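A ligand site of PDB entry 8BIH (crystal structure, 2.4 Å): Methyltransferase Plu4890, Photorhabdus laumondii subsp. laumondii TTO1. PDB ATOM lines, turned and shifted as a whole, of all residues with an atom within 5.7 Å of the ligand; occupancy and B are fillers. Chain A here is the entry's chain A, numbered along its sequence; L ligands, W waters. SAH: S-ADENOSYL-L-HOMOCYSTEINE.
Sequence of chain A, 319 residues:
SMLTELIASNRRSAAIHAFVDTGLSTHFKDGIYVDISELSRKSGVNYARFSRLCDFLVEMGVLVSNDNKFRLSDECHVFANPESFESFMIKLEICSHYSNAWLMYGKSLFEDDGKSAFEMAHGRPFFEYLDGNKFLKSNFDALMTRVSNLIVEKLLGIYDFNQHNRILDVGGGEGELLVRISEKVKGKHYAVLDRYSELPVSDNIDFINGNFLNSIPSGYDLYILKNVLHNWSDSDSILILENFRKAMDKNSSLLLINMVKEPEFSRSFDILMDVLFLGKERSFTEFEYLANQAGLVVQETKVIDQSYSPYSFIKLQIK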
ATOM      1  N   PHE A 127     -10.246 -31.295   2.362  1.00  0.00           N
ATOM      2  CA  PHE A 127      -9.814 -30.888   3.722  1.00  0.00           C
ATOM      3  C   PHE A 127     -10.941 -31.083   4.740  1.00  0.00           C
ATOM      4  O   PHE A 127     -10.645 -31.437   5.891  1.00  0.00           O
ATOM      5  CB  PHE A 127      -9.288 -29.437   3.720  1.00  0.00           C
ATOM      6  CG  PHE A 127      -7.967 -29.274   3.003  1.00  0.00           C
ATOM      7  CD1 PHE A 127      -6.848 -29.964   3.422  1.00  0.00           C
ATOM      8  CD2 PHE A 127      -7.857 -28.432   1.906  1.00  0.00           C
ATOM      9  CE1 PHE A 127      -5.630 -29.813   2.760  1.00  0.00           C
ATOM     10  CE2 PHE A 127      -6.639 -28.268   1.256  1.00  0.00           C
ATOM     11  CZ  PHE A 127      -5.530 -28.971   1.680  1.00  0.00           C
ATOM     12  N   LYS A 137      -5.654 -37.384   7.419  1.00  0.00           N
ATOM     13  CA  LYS A 137      -5.203 -36.091   8.012  1.00  0.00           C
ATOM     14  C   LYS A 137      -3.787 -36.234   8.583  1.00  0.00           C
ATOM     15  O   LYS A 137      -2.962 -35.337   8.305  1.00  0.00           O
ATOM     16  CB  LYS A 137      -6.167 -35.585   9.091  1.00  0.00           C
ATOM     17  CG  LYS A 137      -5.724 -34.292   9.760  1.00  0.00           C
ATOM     18  CD  LYS A 137      -6.832 -33.514  10.429  1.00  0.00           C
ATOM     19  CE  LYS A 137      -6.337 -32.253  11.117  1.00  0.00           C
ATOM     20  NZ  LYS A 137      -5.788 -31.273  10.141  1.00  0.00           N
ATOM     21  N   PHE A 140      -1.127 -36.934   5.719  1.00  0.00           N
ATOM     22  CA  PHE A 140      -1.042 -35.668   4.945  1.00  0.00           C
ATOM     23  C   PHE A 140      -0.252 -34.623   5.749  1.00  0.00           C
ATOM     24  O   PHE A 140       0.759 -34.127   5.233  1.00  0.00           O
ATOM     25  CB  PHE A 140      -2.433 -35.122   4.608  1.00  0.00           C
ATOM     26  CG  PHE A 140      -2.416 -33.854   3.782  1.00  0.00           C
ATOM     27  CD1 PHE A 140      -2.460 -33.912   2.395  1.00  0.00           C
ATOM     28  CD2 PHE A 140      -2.353 -32.614   4.400  1.00  0.00           C
ATOM     29  CE1 PHE A 140      -2.433 -32.745   1.644  1.00  0.00           C
ATOM     30  CE2 PHE A 140      -2.334 -31.450   3.644  1.00  0.00           C
ATOM     31  CZ  PHE A 140      -2.376 -31.517   2.259  1.00  0.00           C
ATOM     32  N   ASP A 141      -0.699 -34.332   6.984  1.00  0.00           N
ATOM     33  CA  ASP A 141      -0.075 -33.313   7.877  1.00  0.00           C
ATOM     34  C   ASP A 141       1.373 -33.709   8.177  1.00  0.00           C
ATOM     35  O   ASP A 141       2.201 -32.786   8.377  1.00  0.00           O
ATOM     36  CB  ASP A 141      -0.892 -33.118   9.159  1.00  0.00           C
ATOM     37  CG  ASP A 141      -2.138 -32.272   8.991  1.00  0.00           C
ATOM     38  OD1 ASP A 141      -2.184 -31.464   8.033  1.00  0.00           O
ATOM     39  OD2 ASP A 141      -3.071 -32.412   9.809  1.00  0.00           O
ATOM     40  N   MET A 144       3.445 -32.898   4.813  1.00  0.00           N
ATOM     41  CA  MET A 144       3.621 -31.430   4.743  1.00  0.00           C
ATOM     42  C   MET A 144       4.700 -30.994   5.742  1.00  0.00           C
ATOM     43  O   MET A 144       5.475 -30.066   5.423  1.00  0.00           O
ATOM     44  CB  MET A 144       2.319 -30.684   5.053  1.00  0.00           C
ATOM     45  CG  MET A 144       1.208 -30.900   4.034  1.00  0.00           C
ATOM     46  SD  MET A 144       1.714 -30.633   2.323  1.00  0.00           S
ATOM     47  CE  MET A 144       1.977 -32.330   1.793  1.00  0.00           C
ATOM     48  N   THR A 145       4.751 -31.644   6.912  1.00  0.00           N
ATOM     49  CA  THR A 145       5.716 -31.364   8.006  1.00  0.00           C
ATOM     50  C   THR A 145       7.146 -31.714   7.552  1.00  0.00           C
ATOM     51  O   THR A 145       8.068 -30.964   7.924  1.00  0.00           O
ATOM     52  CB  THR A 145       5.310 -32.115   9.289  1.00  0.00           C
ATOM     53  OG1 THR A 145       4.131 -31.487   9.787  1.00  0.00           O
ATOM     54  CG2 THR A 145       6.381 -32.105  10.354  1.00  0.00           C
ATOM     55  N   VAL A 147       8.373 -32.009   4.293  1.00  0.00           N
ATOM     56  CA  VAL A 147       8.780 -31.161   3.127  1.00  0.00           C
ATOM     57  C   VAL A 147       9.049 -29.722   3.612  1.00  0.00           C
ATOM     58  O   VAL A 147       9.924 -29.068   3.026  1.00  0.00           O
ATOM     59  CB  VAL A 147       7.756 -31.203   1.985  1.00  0.00           C
ATOM     60  CG1 VAL A 147       7.547 -32.619   1.467  1.00  0.00           C
ATOM     61  CG2 VAL A 147       6.429 -30.567   2.373  1.00  0.00           C
ATOM     62  N   SER A 148       8.312 -29.272   4.640  1.00  0.00           N
ATOM     63  CA  SER A 148       8.488 -27.937   5.290  1.00  0.00           C
ATOM     64  C   SER A 148       9.817 -27.894   6.043  1.00  0.00           C
ATOM     65  O   SER A 148      10.473 -26.842   6.024  1.00  0.00           O
ATOM     66  CB  SER A 148       7.337 -27.616   6.212  1.00  0.00           C
ATOM     67  OG  SER A 148       6.199 -27.228   5.456  1.00  0.00           O
ATOM     68  N   ASP A 169       2.095 -17.658  10.057  1.00  0.00           N
ATOM     69  CA  ASP A 169       2.105 -18.675   8.970  1.00  0.00           C
ATOM     70  C   ASP A 169       0.672 -19.138   8.714  1.00  0.00           C
ATOM     71  O   ASP A 169       0.138 -19.908   9.536  1.00  0.00           O
ATOM     72  CB  ASP A 169       3.029 -19.845   9.308  1.00  0.00           C
ATOM     73  CG  ASP A 169       3.239 -20.821   8.166  1.00  0.00           C
ATOM     74  OD1 ASP A 169       2.824 -20.491   7.025  1.00  0.00           O
ATOM     75  OD2 ASP A 169       3.824 -21.902   8.408  1.00  0.00           O
ATOM     76  N   VAL A 170       0.068 -18.679   7.612  1.00  0.00           N
ATOM     77  CA  VAL A 170      -1.341 -18.979   7.219  1.00  0.00           C
ATOM     78  C   VAL A 170      -1.369 -20.309   6.459  1.00  0.00           C
ATOM     79  O   VAL A 170      -0.632 -20.442   5.477  1.00  0.00           O
ATOM     80  CB  VAL A 170      -1.929 -17.830   6.371  1.00  0.00           C
ATOM     81  CG1 VAL A 170      -3.336 -18.138   5.874  1.00  0.00           C
ATOM     82  CG2 VAL A 170      -1.912 -16.513   7.136  1.00  0.00           C
ATOM     83  N   GLY A 171      -2.212 -21.246   6.901  1.00  0.00           N
ATOM     84  CA  GLY A 171      -2.247 -22.636   6.404  1.00  0.00           C
ATOM     85  C   GLY A 171      -0.964 -23.368   6.722  1.00  0.00           C
ATOM     86  O   GLY A 171      -0.495 -24.153   5.884  1.00  0.00           O
ATOM     87  N   GLY A 172      -0.413 -23.134   7.920  1.00  0.00           N
ATOM     88  CA  GLY A 172       0.926 -23.617   8.342  1.00  0.00           C
ATOM     89  C   GLY A 172       0.915 -25.069   8.789  1.00  0.00           C
ATOM     90  O   GLY A 172       2.012 -25.607   9.032  1.00  0.00           O
ATOM     91  N   GLY A 173      -0.266 -25.683   8.902  1.00  0.00           N
ATOM     92  CA  GLY A 173      -0.432 -27.118   9.246  1.00  0.00           C
ATOM     93  C   GLY A 173      -0.053 -27.394  10.679  1.00  0.00           C
ATOM     94  O   GLY A 173      -0.631 -26.759  11.580  1.00  0.00           O
ATOM     95  N   LEU A 193      -1.697 -20.199  11.692  1.00  0.00           N
ATOM     96  CA  LEU A 193      -3.164 -20.248  11.428  1.00  0.00           C
ATOM     97  C   LEU A 193      -3.481 -21.447  10.542  1.00  0.00           C
ATOM     98  O   LEU A 193      -2.765 -21.644   9.537  1.00  0.00           O
ATOM     99  CB  LEU A 193      -3.589 -18.928  10.769  1.00  0.00           C
ATOM    100  CG  LEU A 193      -5.088 -18.721  10.625  1.00  0.00           C
ATOM    101  CD1 LEU A 193      -5.448 -17.253  10.772  1.00  0.00           C
ATOM    102  CD2 LEU A 193      -5.594 -19.253   9.290  1.00  0.00           C
ATOM    103  N   ASP A 194      -4.524 -22.219  10.889  1.00  0.00           N
ATOM    104  CA  ASP A 194      -5.002 -23.385  10.106  1.00  0.00           C
ATOM    105  C   ASP A 194      -6.376 -23.824  10.629  1.00  0.00           C
ATOM    106  O   ASP A 194      -6.843 -23.242  11.631  1.00  0.00           O
ATOM    107  CB  ASP A 194      -3.988 -24.535  10.173  1.00  0.00           C
ATOM    108  CG  ASP A 194      -3.982 -25.431   8.944  1.00  0.00           C
ATOM    109  OD1 ASP A 194      -4.960 -26.183   8.771  1.00  0.00           O
ATOM    110  OD2 ASP A 194      -2.995 -25.368   8.192  1.00  0.00           O
ATOM    111  N   ARG A 195      -7.010 -24.796   9.951  1.00  0.00           N
ATOM    112  CA  ARG A 195      -8.312 -25.396  10.342  1.00  0.00           C
ATOM    113  C   ARG A 195      -8.054 -26.496  11.378  1.00  0.00           C
ATOM    114  O   ARG A 195      -7.847 -27.655  10.978  1.00  0.00           O
ATOM    115  CB  ARG A 195      -9.050 -25.939   9.114  1.00  0.00           C
ATOM    116  CG  ARG A 195      -9.493 -24.855   8.131  1.00  0.00           C
ATOM    117  CD  ARG A 195     -10.185 -25.425   6.908  1.00  0.00           C
ATOM    118  NE  ARG A 195     -11.492 -26.010   7.214  1.00  0.00           N
ATOM    119  CZ  ARG A 195     -11.704 -27.293   7.484  1.00  0.00           C
ATOM    120  NH1 ARG A 195     -10.719 -28.172   7.510  1.00  0.00           N
ATOM    121  NH2 ARG A 195     -12.939 -27.703   7.752  1.00  0.00           N
ATOM    122  N   GLY A 210      -8.694 -21.053  12.382  1.00  0.00           N
ATOM    123  CA  GLY A 210      -9.270 -20.038  11.483  1.00  0.00           C
ATOM    124  C   GLY A 210      -9.510 -20.584  10.085  1.00  0.00           C
ATOM    125  O   GLY A 210      -9.244 -21.777   9.860  1.00  0.00           O
ATOM    126  N   ASN A 211      -9.994 -19.708   9.194  1.00  0.00           N
ATOM    127  CA  ASN A 211     -10.339 -20.014   7.781  1.00  0.00           C
ATOM    128  C   ASN A 211      -9.936 -18.814   6.915  1.00  0.00           C
ATOM    129  O   ASN A 211     -10.604 -17.759   7.020  1.00  0.00           O
ATOM    130  CB  ASN A 211     -11.830 -20.343   7.653  1.00  0.00           C
ATOM    131  CG  ASN A 211     -12.272 -20.607   6.229  1.00  0.00           C
ATOM    132  OD1 ASN A 211     -11.460 -20.588   5.303  1.00  0.00           O
ATOM    133  ND2 ASN A 211     -13.551 -20.859   6.041  1.00  0.00           N
ATOM    134  N   PHE A 212      -8.889 -18.969   6.094  1.00  0.00           N
ATOM    135  CA  PHE A 212      -8.274 -17.871   5.296  1.00  0.00           C
ATOM    136  C   PHE A 212      -9.234 -17.373   4.204  1.00  0.00           C
ATOM    137  O   PHE A 212      -8.919 -16.346   3.589  1.00  0.00           O
ATOM    138  CB  PHE A 212      -6.911 -18.256   4.709  1.00  0.00           C
ATOM    139  CG  PHE A 212      -6.805 -19.599   4.005  1.00  0.00           C
ATOM    140  CD1 PHE A 212      -5.768 -20.460   4.329  1.00  0.00           C
ATOM    141  CD2 PHE A 212      -7.690 -19.964   3.004  1.00  0.00           C
ATOM    142  CE1 PHE A 212      -5.634 -21.677   3.676  1.00  0.00           C
ATOM    143  CE2 PHE A 212      -7.556 -21.182   2.351  1.00  0.00           C
ATOM    144  CZ  PHE A 212      -6.530 -22.043   2.692  1.00  0.00           C
ATOM    145  N   LEU A 213     -10.349 -18.085   3.962  1.00  0.00           N
ATOM    146  CA  LEU A 213     -11.418 -17.692   3.004  1.00  0.00           C
ATOM    147  C   LEU A 213     -12.290 -16.602   3.637  1.00  0.00           C
ATOM    148  O   LEU A 213     -12.762 -15.715   2.905  1.00  0.00           O
ATOM    149  CB  LEU A 213     -12.258 -18.918   2.622  1.00  0.00           C
ATOM    150  CG  LEU A 213     -11.518 -20.040   1.922  1.00  0.00           C
ATOM    151  CD1 LEU A 213     -12.371 -21.297   1.858  1.00  0.00           C
ATOM    152  CD2 LEU A 213     -11.089 -19.622   0.525  1.00  0.00           C
ATOM    153  N   LYS A 226       2.740 -20.793   2.372  1.00  0.00           N
ATOM    154  CA  LYS A 226       3.546 -21.847   1.699  1.00  0.00           C
ATOM    155  C   LYS A 226       2.635 -23.024   1.299  1.00  0.00           C
ATOM    156  O   LYS A 226       1.946 -23.553   2.193  1.00  0.00           O
ATOM    157  CB  LYS A 226       4.691 -22.334   2.598  1.00  0.00           C
ATOM    158  CG  LYS A 226       5.737 -23.180   1.893  1.00  0.00           C
ATOM    159  CD  LYS A 226       6.941 -23.508   2.746  1.00  0.00           C
ATOM    160  CE  LYS A 226       6.735 -24.699   3.670  1.00  0.00           C
ATOM    161  NZ  LYS A 226       6.833 -25.985   2.938  1.00  0.00           N
ATOM    162  N   ASN A 227       2.660 -23.401   0.024  1.00  0.00           N
ATOM    163  CA  ASN A 227       1.999 -24.617  -0.542  1.00  0.00           C
ATOM    164  C   ASN A 227       0.511 -24.614  -0.203  1.00  0.00           C
ATOM    165  O   ASN A 227      -0.003 -25.644   0.271  1.00  0.00           O
ATOM    166  CB  ASN A 227       2.687 -25.907  -0.053  1.00  0.00           C
ATOM    167  CG  ASN A 227       4.029 -26.155  -0.723  1.00  0.00           C
ATOM    168  OD1 ASN A 227       4.403 -25.457  -1.664  1.00  0.00           O
ATOM    169  ND2 ASN A 227       4.752 -27.160  -0.248  1.00  0.00           N
ATOM    170  N   VAL A 228      -0.171 -23.491  -0.456  1.00  0.00           N
ATOM    171  CA  VAL A 228      -1.622 -23.299  -0.189  1.00  0.00           C
ATOM    172  C   VAL A 228      -2.359 -23.084  -1.520  1.00  0.00           C
ATOM    173  O   VAL A 228      -3.288 -23.852  -1.804  1.00  0.00           O
ATOM    174  CB  VAL A 228      -1.877 -22.115   0.776  1.00  0.00           C
ATOM    175  CG1 VAL A 228      -3.344 -21.730   0.848  1.00  0.00           C
ATOM    176  CG2 VAL A 228      -1.325 -22.410   2.161  1.00  0.00           C
ATOM    177  N   HIS A 230      -2.064 -23.659  -4.612  1.00  0.00           N
ATOM    178  CA  HIS A 230      -2.179 -24.754  -5.621  1.00  0.00           C
ATOM    179  C   HIS A 230      -3.321 -25.715  -5.264  1.00  0.00           C
ATOM    180  O   HIS A 230      -3.570 -26.642  -6.062  1.00  0.00           O
ATOM    181  CB  HIS A 230      -0.831 -25.486  -5.811  1.00  0.00           C
ATOM    182  CG  HIS A 230      -0.265 -26.137  -4.592  1.00  0.00           C
ATOM    183  ND1 HIS A 230      -1.028 -26.436  -3.487  1.00  0.00           N
ATOM    184  CD2 HIS A 230       0.975 -26.582  -4.322  1.00  0.00           C
ATOM    185  CE1 HIS A 230      -0.272 -27.021  -2.573  1.00  0.00           C
ATOM    186  NE2 HIS A 230       0.962 -27.119  -3.063  1.00  0.00           N
ATOM    187  N   ASN A 231      -3.993 -25.512  -4.128  1.00  0.00           N
ATOM    188  CA  ASN A 231      -5.177 -26.299  -3.678  1.00  0.00           C
ATOM    189  C   ASN A 231      -6.483 -25.544  -3.952  1.00  0.00           C
ATOM    190  O   ASN A 231      -7.533 -25.992  -3.447  1.00  0.00           O
ATOM    191  CB  ASN A 231      -5.096 -26.647  -2.189  1.00  0.00           C
ATOM    192  CG  ASN A 231      -3.838 -27.398  -1.816  1.00  0.00           C
ATOM    193  OD1 ASN A 231      -3.250 -28.101  -2.641  1.00  0.00           O
ATOM    194  ND2 ASN A 231      -3.414 -27.258  -0.565  1.00  0.00           N
ATOM    195  N   TRP A 232      -6.449 -24.440  -4.711  1.00  0.00           N
ATOM    196  CA  TRP A 232      -7.622 -23.530  -4.883  1.00  0.00           C
ATOM    197  C   TRP A 232      -7.660 -22.929  -6.289  1.00  0.00           C
ATOM    198  O   TRP A 232      -6.580 -22.736  -6.893  1.00  0.00           O
ATOM    199  CB  TRP A 232      -7.596 -22.430  -3.810  1.00  0.00           C
ATOM    200  CG  TRP A 232      -7.445 -22.955  -2.418  1.00  0.00           C
ATOM    201  CD1 TRP A 232      -6.291 -23.036  -1.700  1.00  0.00           C
ATOM    202  CD2 TRP A 232      -8.473 -23.504  -1.586  1.00  0.00           C
ATOM    203  NE1 TRP A 232      -6.534 -23.597  -0.472  1.00  0.00           N
ATOM    204  CE2 TRP A 232      -7.862 -23.898  -0.375  1.00  0.00           C
ATOM    205  CE3 TRP A 232      -9.858 -23.709  -1.732  1.00  0.00           C
ATOM    206  CZ2 TRP A 232      -8.581 -24.460   0.675  1.00  0.00           C
ATOM    207  CZ3 TRP A 232     -10.564 -24.280  -0.698  1.00  0.00           C
ATOM    208  CH2 TRP A 232      -9.935 -24.652   0.488  1.00  0.00           C
HETATM  209  N   SAH L   1       1.750 -24.654   4.622  1.00  0.00           N
HETATM  210  CA  SAH L   1       2.012 -26.072   5.022  1.00  0.00           C
HETATM  211  CB  SAH L   1       0.824 -26.977   4.666  1.00  0.00           C
HETATM  212  CG  SAH L   1       0.416 -26.930   3.193  1.00  0.00           C
HETATM  213  SD  SAH L   1      -0.939 -28.061   2.820  1.00  0.00           S
HETATM  214  C   SAH L   1       3.271 -26.585   4.326  1.00  0.00           C
HETATM  215  O   SAH L   1       3.806 -27.634   4.713  1.00  0.00           O
HETATM  216  OXT SAH L   1       3.776 -25.985   3.381  1.00  0.00           O
HETATM  217  C5' SAH L   1      -2.397 -26.970   2.897  1.00  0.00           C
HETATM  218  C4' SAH L   1      -2.852 -26.588   4.290  1.00  0.00           C
HETATM  219  O4' SAH L   1      -3.918 -25.626   4.216  1.00  0.00           O
HETATM  220  C3' SAH L   1      -3.381 -27.756   5.139  1.00  0.00           C
HETATM  221  O3' SAH L   1      -2.624 -27.884   6.331  1.00  0.00           O
HETATM  222  C2' SAH L   1      -4.839 -27.383   5.414  1.00  0.00           C
HETATM  223  O2' SAH L   1      -5.288 -27.753   6.706  1.00  0.00           O
HETATM  224  C1' SAH L   1      -4.807 -25.866   5.282  1.00  0.00           C
HETATM  225  N9  SAH L   1      -6.095 -25.251   4.972  1.00  0.00           N
HETATM  226  C8  SAH L   1      -7.005 -25.695   4.049  1.00  0.00           C
HETATM  227  N7  SAH L   1      -8.081 -24.939   3.970  1.00  0.00           N
HETATM  228  C5  SAH L   1      -7.849 -23.931   4.886  1.00  0.00           C
HETATM  229  C6  SAH L   1      -8.611 -22.811   5.271  1.00  0.00           C
HETATM  230  N6  SAH L   1      -9.797 -22.513   4.743  1.00  0.00           N
HETATM  231  N1  SAH L   1      -8.084 -21.983   6.211  1.00  0.00           N
HETATM  232  C2  SAH L   1      -6.890 -22.291   6.733  1.00  0.00           C
HETATM  233  N3  SAH L   1      -6.092 -23.317   6.450  1.00  0.00           N
HETATM  234  C4  SAH L   1      -6.626 -24.114   5.518  1.00  0.00           C
HETATM  235  O   HOH W   1      -5.024 -25.559   1.213  1.00  0.00           O
HETATM  236  O   HOH W   2       1.810 -21.592   4.971  1.00  0.00           O
HETATM  237  O   HOH W   3      -0.712 -29.772   6.639  1.00  0.00           O
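The backbone carbonyl oxygen (O) of Lys 226 lies within hydrogen-bond range of a nitrogen (N) of the ligand, at 2.7 Å.
The side-chain carboxylate of Asp 194 lies within hydrogen-bond range of an oxygen (O2') of the ligand, 2.6 Å away.
The backbone NH of Phe 212 lies within hydrogen-bond range of a nitrogen (N1) of the ligand.
OG of Ser 148 is in hydrogen-bond range of O of the ligand (2.5 Å).
The backbone carbonyl oxygen of Gly 171 lies within hydrogen-bond range of a nitrogen (N) of the ligand (2.6 Å).
O of the ligand sits close to O of Met 144 (3.0 Å).
An oxygen (OXT) of the ligand is in salt-bridge range of the side-chain amino group (NZ) of Lys 226, at 3.1 Å.
The side-chain amide oxygen of Asn 211 lies within hydrogen-bond range of a nitrogen (N6) of the ligand, at 2.6 Å.
OG of Ser 148 sits at hydrogen-bond distance from NZ of Lys 226, 2.9 Å away.
ND1 of His 230 is in hydrogen-bond range of OD1 of Asn 231, 2.9 Å away.
O of Leu 193 lies within hydrogen-bond range of N of Gly 171 (2.7 Å).
The backbone NH of Leu 213 lies within hydrogen-bond range of the side-chain amide oxygen of Asn 211 (3.0 Å).
The backbone carbonyl oxygen (O) of Asp 194 lies within hydrogen-bond range of the backbone NH (N) of Gly 210, at 3.0 Å.
The side-chain hydroxyl of Ser 148 is in hydrogen-bond range of the backbone carbonyl oxygen of Met 144 (2.9 Å).
The backbone NH of Gly 172 lies within hydrogen-bond range of the backbone carbonyl oxygen of Leu 193.
N of Gly 172 lies within hydrogen-bond range of OD2 of Asp 194 (3.4 Å).
The backbone carbonyl oxygen of Asn 227 lies close to a sulfur (SD) of the ligand, 3.6 Å away.
CD2 of Phe 127 touches C8 of the ligand, at 3.6 Å.
Phe 140 touches the ligand (CE2 to SD, 3.8 Å).
OD1 of Asp 141 touches O3' of the ligand, at 3.99 Å.
Gly 172 touches the ligand.
Gly 173 touches the ligand (CA to O3', 3.7 Å).
CD of Arg 195 touches C5 of the ligand, at 3.4 Å.
Gly 210 touches the ligand.
ND2 of Asn 231 touches C5' of the ligand, at 3.6 Å.
Trp 232 touches the ligand.
Hydrophobic or aromatic side chains within 4 Å of the ligand: Phe 127, Phe 140, Met 144, Phe 212 and Trp 232.
Of the 26 residues printed, 17 come within 4 Å of the ligand.
Water W3 lies within hydrogen-bond range of OD1 of Asp 141 (2.6 Å) and O3' of the ligand (2.7 Å).
Water W2 lies within hydrogen-bond range of OD1 of Asp 169 (2.5 Å), O of Val 170 (2.7 Å), N of Lys 226 (2.9 Å) and N of the ligand (3.1 Å).
Water W1 lies within hydrogen-bond range of the side-chain amide nitrogen of Asn 231 (2.9 Å), the indole nitrogen of Trp 232 (3.0 Å) and an oxygen (O4') of the ligand (3.2 Å).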
